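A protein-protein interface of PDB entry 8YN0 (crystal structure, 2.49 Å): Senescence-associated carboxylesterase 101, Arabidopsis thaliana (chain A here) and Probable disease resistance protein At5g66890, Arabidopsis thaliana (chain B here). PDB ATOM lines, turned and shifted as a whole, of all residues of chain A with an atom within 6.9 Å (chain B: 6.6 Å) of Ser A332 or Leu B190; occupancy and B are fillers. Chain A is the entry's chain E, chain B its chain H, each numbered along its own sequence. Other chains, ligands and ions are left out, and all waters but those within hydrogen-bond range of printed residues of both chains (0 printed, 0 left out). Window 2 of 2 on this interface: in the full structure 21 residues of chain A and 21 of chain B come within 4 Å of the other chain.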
ATOM      1  N   ARG A 323      22.862 -21.091  34.181  1.00  0.00           N
ATOM      2  CA  ARG A 323      22.490 -21.095  32.807  1.00  0.00           C
ATOM      3  C   ARG A 323      21.631 -22.257  32.550  1.00  0.00           C
ATOM      4  O   ARG A 323      20.661 -22.154  31.852  1.00  0.00           O
ATOM      5  CB  ARG A 323      23.726 -21.218  31.951  1.00  0.00           C
ATOM      6  CG  ARG A 323      23.470 -21.483  30.488  1.00  0.00           C
ATOM      7  CD  ARG A 323      23.169 -20.217  29.726  1.00  0.00           C
ATOM      8  NE  ARG A 323      23.039 -20.515  28.312  1.00  0.00           N
ATOM      9  CZ  ARG A 323      23.311 -19.668  27.334  1.00  0.00           C
ATOM     10  NH1 ARG A 323      23.746 -18.453  27.606  1.00  0.00           N
ATOM     11  NH2 ARG A 323      23.167 -20.047  26.083  1.00  0.00           N
ATOM     12  N   THR A 326      18.212 -21.242  34.263  1.00  0.00           N
ATOM     13  CA  THR A 326      17.572 -20.188  33.485  1.00  0.00           C
ATOM     14  C   THR A 326      17.028 -20.710  32.172  1.00  0.00           C
ATOM     15  O   THR A 326      15.857 -20.494  31.835  1.00  0.00           O
ATOM     16  CB  THR A 326      18.582 -19.088  33.213  1.00  0.00           C
ATOM     17  OG1 THR A 326      19.111 -18.628  34.466  1.00  0.00           O
ATOM     18  CG2 THR A 326      17.917 -17.945  32.455  1.00  0.00           C
ATOM     19  N   GLN A 327      17.884 -21.376  31.402  1.00  0.00           N
ATOM     20  CA  GLN A 327      17.496 -21.868  30.094  1.00  0.00           C
ATOM     21  C   GLN A 327      16.421 -22.941  30.190  1.00  0.00           C
ATOM     22  O   GLN A 327      15.618 -23.087  29.267  1.00  0.00           O
ATOM     23  CB  GLN A 327      18.741 -22.386  29.383  1.00  0.00           C
ATOM     24  CG  GLN A 327      18.677 -22.289  27.883  1.00  0.00           C
ATOM     25  CD  GLN A 327      18.519 -20.884  27.397  1.00  0.00           C
ATOM     26  OE1 GLN A 327      17.674 -20.628  26.576  1.00  0.00           O
ATOM     27  NE2 GLN A 327      19.320 -19.962  27.909  1.00  0.00           N
ATOM     28  N   PHE A 330      13.267 -20.730  30.890  1.00  0.00           N
ATOM     29  CA  PHE A 330      12.966 -19.859  29.759  1.00  0.00           C
ATOM     30  C   PHE A 330      13.846 -20.236  28.573  1.00  0.00           C
ATOM     31  O   PHE A 330      14.882 -19.612  28.318  1.00  0.00           O
ATOM     32  CB  PHE A 330      13.126 -18.395  30.155  1.00  0.00           C
ATOM     33  CG  PHE A 330      12.184 -17.971  31.247  1.00  0.00           C
ATOM     34  CD1 PHE A 330      10.861 -17.648  30.950  1.00  0.00           C
ATOM     35  CD2 PHE A 330      12.612 -17.919  32.570  1.00  0.00           C
ATOM     36  CE1 PHE A 330       9.981 -17.268  31.949  1.00  0.00           C
ATOM     37  CE2 PHE A 330      11.736 -17.535  33.585  1.00  0.00           C
ATOM     38  CZ  PHE A 330      10.415 -17.210  33.273  1.00  0.00           C
ATOM     39  N   PRO A 331      13.446 -21.242  27.810  1.00  0.00           N
ATOM     40  CA  PRO A 331      14.279 -21.703  26.692  1.00  0.00           C
ATOM     41  C   PRO A 331      14.444 -20.633  25.621  1.00  0.00           C
ATOM     42  O   PRO A 331      13.471 -20.064  25.134  1.00  0.00           O
ATOM     43  CB  PRO A 331      13.504 -22.915  26.157  1.00  0.00           C
ATOM     44  CG  PRO A 331      12.597 -23.343  27.289  1.00  0.00           C
ATOM     45  CD  PRO A 331      12.239 -22.068  28.007  1.00  0.00           C
ATOM     46  N   SER A 332      15.694 -20.365  25.250  1.00  0.00           N
ATOM     47  CA  SER A 332      15.967 -19.486  24.123  1.00  0.00           C
ATOM     48  C   SER A 332      17.159 -19.896  23.264  1.00  0.00           C
ATOM     49  O   SER A 332      17.294 -19.344  22.170  1.00  0.00           O
ATOM     50  CB  SER A 332      16.177 -18.039  24.595  1.00  0.00           C
ATOM     51  OG  SER A 332      17.289 -17.936  25.453  1.00  0.00           O
ATOM     52  N   LYS A 333      17.997 -20.855  23.670  1.00  0.00           N
ATOM     53  CA  LYS A 333      19.131 -21.273  22.849  1.00  0.00           C
ATOM     54  C   LYS A 333      19.165 -22.789  22.684  1.00  0.00           C
ATOM     55  O   LYS A 333      18.797 -23.546  23.586  1.00  0.00           O
ATOM     56  CB  LYS A 333      20.479 -20.770  23.429  1.00  0.00           C
ATOM     57  CG  LYS A 333      20.645 -19.212  23.446  1.00  0.00           C
ATOM     58  CD  LYS A 333      20.516 -18.599  22.060  1.00  0.00           C
ATOM     59  CE  LYS A 333      21.312 -17.289  21.869  1.00  0.00           C
ATOM     60  NZ  LYS A 333      21.869 -17.198  20.445  1.00  0.00           N
ATOM     61  N   GLU A 334      19.640 -23.230  21.516  1.00  0.00           N
ATOM     62  CA  GLU A 334      19.566 -24.646  21.136  1.00  0.00           C
ATOM     63  C   GLU A 334      20.639 -25.489  21.811  1.00  0.00           C
ATOM     64  O   GLU A 334      20.404 -26.660  22.146  1.00  0.00           O
ATOM     65  CB  GLU A 334      19.680 -24.790  19.613  1.00  0.00           C
ATOM     66  CG  GLU A 334      18.516 -24.188  18.873  1.00  0.00           C
ATOM     67  CD  GLU A 334      18.728 -22.719  18.502  1.00  0.00           C
ATOM     68  OE1 GLU A 334      19.598 -22.025  19.080  1.00  0.00           O
ATOM     69  OE2 GLU A 334      18.003 -22.262  17.603  1.00  0.00           O
ATOM     70  N   ASP A 336      21.789 -25.441  24.762  1.00  0.00           N
ATOM     71  CA  ASP A 336      21.396 -25.860  26.099  1.00  0.00           C
ATOM     72  C   ASP A 336      20.387 -26.993  26.036  1.00  0.00           C
ATOM     73  O   ASP A 336      20.412 -27.915  26.869  1.00  0.00           O
ATOM     74  CB  ASP A 336      20.804 -24.678  26.868  1.00  0.00           C
ATOM     75  CG  ASP A 336      21.765 -23.524  26.989  1.00  0.00           C
ATOM     76  OD1 ASP A 336      22.062 -22.889  25.975  1.00  0.00           O
ATOM     77  OD2 ASP A 336      22.243 -23.256  28.099  1.00  0.00           O
ATOM     78  N   ILE A 337      19.467 -26.923  25.074  1.00  0.00           N
ATOM     79  CA  ILE A 337      18.468 -27.967  24.952  1.00  0.00           C
ATOM     80  C   ILE A 337      19.139 -29.272  24.611  1.00  0.00           C
ATOM     81  O   ILE A 337      18.710 -30.338  25.080  1.00  0.00           O
ATOM     82  CB  ILE A 337      17.412 -27.575  23.915  1.00  0.00           C
ATOM     83  CG1 ILE A 337      16.376 -26.674  24.592  1.00  0.00           C
ATOM     84  CG2 ILE A 337      16.795 -28.826  23.273  1.00  0.00           C
ATOM     85  CD1 ILE A 337      15.467 -26.013  23.649  1.00  0.00           C
ATOM     86  N   SER B 164      13.160  -8.134  17.520  1.00  0.00           N
ATOM     87  CA  SER B 164      13.626  -8.336  18.883  1.00  0.00           C
ATOM     88  C   SER B 164      12.585  -8.065  19.979  1.00  0.00           C
ATOM     89  O   SER B 164      12.948  -7.950  21.121  1.00  0.00           O
ATOM     90  CB  SER B 164      14.888  -7.536  19.101  1.00  0.00           C
ATOM     91  OG  SER B 164      15.917  -8.024  18.288  1.00  0.00           O
ATOM     92  N   ASN B 187      13.182 -13.999  15.456  1.00  0.00           N
ATOM     93  CA  ASN B 187      13.280 -13.201  16.658  1.00  0.00           C
ATOM     94  C   ASN B 187      14.609 -13.386  17.319  1.00  0.00           C
ATOM     95  O   ASN B 187      15.031 -14.488  17.548  1.00  0.00           O
ATOM     96  CB  ASN B 187      12.155 -13.539  17.628  1.00  0.00           C
ATOM     97  CG  ASN B 187      12.344 -12.937  19.001  1.00  0.00           C
ATOM     98  OD1 ASN B 187      12.670 -11.771  19.142  1.00  0.00           O
ATOM     99  ND2 ASN B 187      12.114 -13.737  20.025  1.00  0.00           N
ATOM    100  N   HIS B 188      15.299 -12.282  17.526  1.00  0.00           N
ATOM    101  CA  HIS B 188      16.588 -12.290  18.177  1.00  0.00           C
ATOM    102  C   HIS B 188      16.513 -11.950  19.625  1.00  0.00           C
ATOM    103  O   HIS B 188      17.505 -12.008  20.338  1.00  0.00           O
ATOM    104  CB  HIS B 188      17.489 -11.340  17.422  1.00  0.00           C
ATOM    105  CG  HIS B 188      17.475 -11.559  15.940  1.00  0.00           C
ATOM    106  ND1 HIS B 188      18.344 -12.364  15.327  1.00  0.00           N
ATOM    107  CD2 HIS B 188      16.645 -11.054  14.951  1.00  0.00           C
ATOM    108  CE1 HIS B 188      18.092 -12.372  14.015  1.00  0.00           C
ATOM    109  NE2 HIS B 188      17.050 -11.573  13.788  1.00  0.00           N
ATOM    110  N   GLY B 189      15.348 -11.621  20.097  1.00  0.00           N
ATOM    111  CA  GLY B 189      15.130 -11.327  21.488  1.00  0.00           C
ATOM    112  C   GLY B 189      15.113 -12.453  22.475  1.00  0.00           C
ATOM    113  O   GLY B 189      14.970 -13.593  22.092  1.00  0.00           O
ATOM    114  N   LEU B 190      15.303 -12.139  23.744  1.00  0.00           N
ATOM    115  CA  LEU B 190      15.261 -13.143  24.804  1.00  0.00           C
ATOM    116  C   LEU B 190      13.941 -13.836  24.954  1.00  0.00           C
ATOM    117  O   LEU B 190      13.873 -15.028  25.153  1.00  0.00           O
ATOM    118  CB  LEU B 190      15.515 -12.446  26.109  1.00  0.00           C
ATOM    119  CG  LEU B 190      15.801 -13.372  27.284  1.00  0.00           C
ATOM    120  CD1 LEU B 190      17.206 -13.931  27.144  1.00  0.00           C
ATOM    121  CD2 LEU B 190      15.647 -12.607  28.584  1.00  0.00           C
ATOM    122  N   GLU B 191      12.882 -13.074  24.845  1.00  0.00           N
ATOM    123  CA  GLU B 191      11.579 -13.641  24.961  1.00  0.00           C
ATOM    124  C   GLU B 191      10.965 -13.998  23.644  1.00  0.00           C
ATOM    125  O   GLU B 191      11.159 -13.311  22.666  1.00  0.00           O
ATOM    126  CB  GLU B 191      10.663 -12.656  25.669  1.00  0.00           C
ATOM    127  CG  GLU B 191      11.139 -12.146  27.003  1.00  0.00           C
ATOM    128  CD  GLU B 191      10.381 -10.906  27.416  1.00  0.00           C
ATOM    129  OE1 GLU B 191       9.201 -11.023  27.794  1.00  0.00           O
ATOM    130  OE2 GLU B 191      10.964  -9.808  27.345  1.00  0.00           O
ATOM    131  N   PRO B 192      10.254 -15.115  23.610  1.00  0.00           N
ATOM    132  CA  PRO B 192       9.492 -15.447  22.402  1.00  0.00           C
ATOM    133  C   PRO B 192       8.632 -14.262  21.993  1.00  0.00           C
ATOM    134  O   PRO B 192       7.860 -13.730  22.793  1.00  0.00           O
ATOM    135  CB  PRO B 192       8.640 -16.649  22.840  1.00  0.00           C
ATOM    136  CG  PRO B 192       9.362 -17.236  24.004  1.00  0.00           C
ATOM    137  CD  PRO B 192      10.122 -16.125  24.676  1.00  0.00           C
ATOM    138  N   LYS B 214      11.599 -18.695  16.883  1.00  0.00           N
ATOM    139  CA  LYS B 214      11.604 -18.176  18.253  1.00  0.00           C
ATOM    140  C   LYS B 214      10.516 -17.124  18.431  1.00  0.00           C
ATOM    141  O   LYS B 214      10.712 -16.104  19.100  1.00  0.00           O
ATOM    142  CB  LYS B 214      12.963 -17.606  18.640  1.00  0.00           C
ATOM    143  CG  LYS B 214      14.076 -18.619  18.898  1.00  0.00           C
ATOM    144  CD  LYS B 214      15.413 -17.902  18.847  1.00  0.00           C
ATOM    145  CE  LYS B 214      16.576 -18.664  19.459  1.00  0.00           C
ATOM    146  NZ  LYS B 214      16.800 -19.963  18.844  1.00  0.00           N
ATOM    147  N   PHE B 237      12.071 -23.308  17.111  1.00  0.00           N
ATOM    148  CA  PHE B 237      12.243 -22.797  18.466  1.00  0.00           C
ATOM    149  C   PHE B 237      11.096 -21.906  18.811  1.00  0.00           C
ATOM    150  O   PHE B 237      11.266 -20.919  19.427  1.00  0.00           O
ATOM    151  CB  PHE B 237      13.621 -22.161  18.674  1.00  0.00           C
ATOM    152  CG  PHE B 237      14.212 -22.378  20.025  1.00  0.00           C
ATOM    153  CD1 PHE B 237      13.588 -21.919  21.159  1.00  0.00           C
ATOM    154  CD2 PHE B 237      15.428 -22.995  20.150  1.00  0.00           C
ATOM    155  CE1 PHE B 237      14.148 -22.106  22.397  1.00  0.00           C
ATOM    156  CE2 PHE B 237      15.998 -23.182  21.380  1.00  0.00           C
ATOM    157  CZ  PHE B 237      15.356 -22.736  22.508  1.00  0.00           C
ATOM    158  N   TYR B 266       9.616 -26.488  22.203  1.00  0.00           N
ATOM    159  CA  TYR B 266       9.818 -27.122  23.500  1.00  0.00           C
ATOM    160  C   TYR B 266       8.533 -27.292  24.306  1.00  0.00           C
ATOM    161  O   TYR B 266       8.512 -28.134  25.209  1.00  0.00           O
ATOM    162  CB  TYR B 266      10.835 -26.309  24.312  1.00  0.00           C
ATOM    163  CG  TYR B 266      10.533 -24.830  24.238  1.00  0.00           C
ATOM    164  CD1 TYR B 266       9.632 -24.243  25.131  1.00  0.00           C
ATOM    165  CD2 TYR B 266      11.090 -24.034  23.237  1.00  0.00           C
ATOM    166  CE1 TYR B 266       9.324 -22.901  25.056  1.00  0.00           C
ATOM    167  CE2 TYR B 266      10.793 -22.669  23.150  1.00  0.00           C
ATOM    168  CZ  TYR B 266       9.910 -22.117  24.059  1.00  0.00           C
ATOM    169  OH  TYR B 266       9.597 -20.805  23.977  1.00  0.00           O
ATOM    170  N   LEU B 414      25.130 -21.859  18.489  1.00  0.00           N
ATOM    171  CA  LEU B 414      23.771 -21.663  18.982  1.00  0.00           C
ATOM    172  C   LEU B 414      23.730 -21.617  20.507  1.00  0.00           C
ATOM    173  O   LEU B 414      22.947 -22.300  21.111  1.00  0.00           O
ATOM    174  CB  LEU B 414      22.855 -22.723  18.384  1.00  0.00           C
ATOM    175  CG  LEU B 414      22.871 -22.857  16.873  1.00  0.00           C
ATOM    176  CD1 LEU B 414      21.893 -23.929  16.448  1.00  0.00           C
ATOM    177  CD2 LEU B 414      22.509 -21.532  16.247  1.00  0.00           C
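NZ of Lys B214 sits close to O of Ser A332 (3.4 Å). The side-chain amino group of Lys B214 lies within salt-bridge range of the side-chain carboxylate of Glu A334 (2.9 Å). The backbone NH (N) of Glu A334 lies within hydrogen-bond range of the backbone carbonyl oxygen (O) of Leu B414, at 3.5 Å.
The side-chain amide oxygen (OE1) of Gln A327 lies within hydrogen-bond range of the side-chain hydroxyl (OG) of Ser A332. The backbone NH (N) of Lys A333 is in hydrogen-bond range of the side-chain amide oxygen (OE1) of Gln A327, 2.9 Å away. The backbone carbonyl oxygen (O) of Lys B214 is in hydrogen-bond range of the side-chain amide nitrogen (ND2) of Asn B187, at 2.9 Å. The backbone NH of Lys B214 sits close to the backbone carbonyl oxygen of Phe B237 (3.4 Å).
CE1 of Phe B237 touches O of Pro A331, at 3.5 Å. Tyr B266 touches Pro A331. O of Leu B190 touches CB of Ser A332 (3.8 Å). CZ of Phe B237 touches C of Ser A332 (3.4 Å). Phe B237 touches Lys A333. Leu B414 touches Lys A333 (O to CB, 3.7 Å). Phe B237 touches Glu A334. CZ of Phe B237 touches CD1 of Ile A337, at 3.5 Å.
Of chain B, only Leu B190, Lys B214 and Phe B237 come within 4 Å of Ser A332. Of chain A, only Ser A332 (3.8 Å) comes within 4 Å of Leu B190. Printed residues of chain A within 4 Å of Leu B414: Lys A333 (3.7 Å) and Glu A334 (3.4 Å). Of the printed residues of chain A, Lys B214 touches Ser A332 and Glu A334. Of the printed residues of chain B, Pro A331 touches Phe B237 (3.5 Å) and Tyr B266 (3.8 Å). Glu B191 touches none of the printed residues of chain A. The nearest residue of chain A that does not touch Leu B190 is Pro A331 (5.1 Å).
Printed residues of chain A that touch a printed residue of chain B: Pro A331, Ser A332, Lys A333, Glu A334 and Ile A337. Hydrophobic or aromatic side chains of chain A that line the printed part of chain B: Pro A331 and Ile A337. Hydrophobic or aromatic side chains of chain B within 4 Å of the printed part of chain A: Phe B237, Tyr B266 and Leu B414. Along chain B the printed residues that touch a printed residue of chain A span positions 190 to 414. Among the printed residues, 11 pairs touch across the chains. Among the printed residues, Asp or Glu carboxylates within 4 Å of a Lys or Arg side-chain nitrogen of the other chain: Glu A334 with Lys B214 (2.9 Å).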
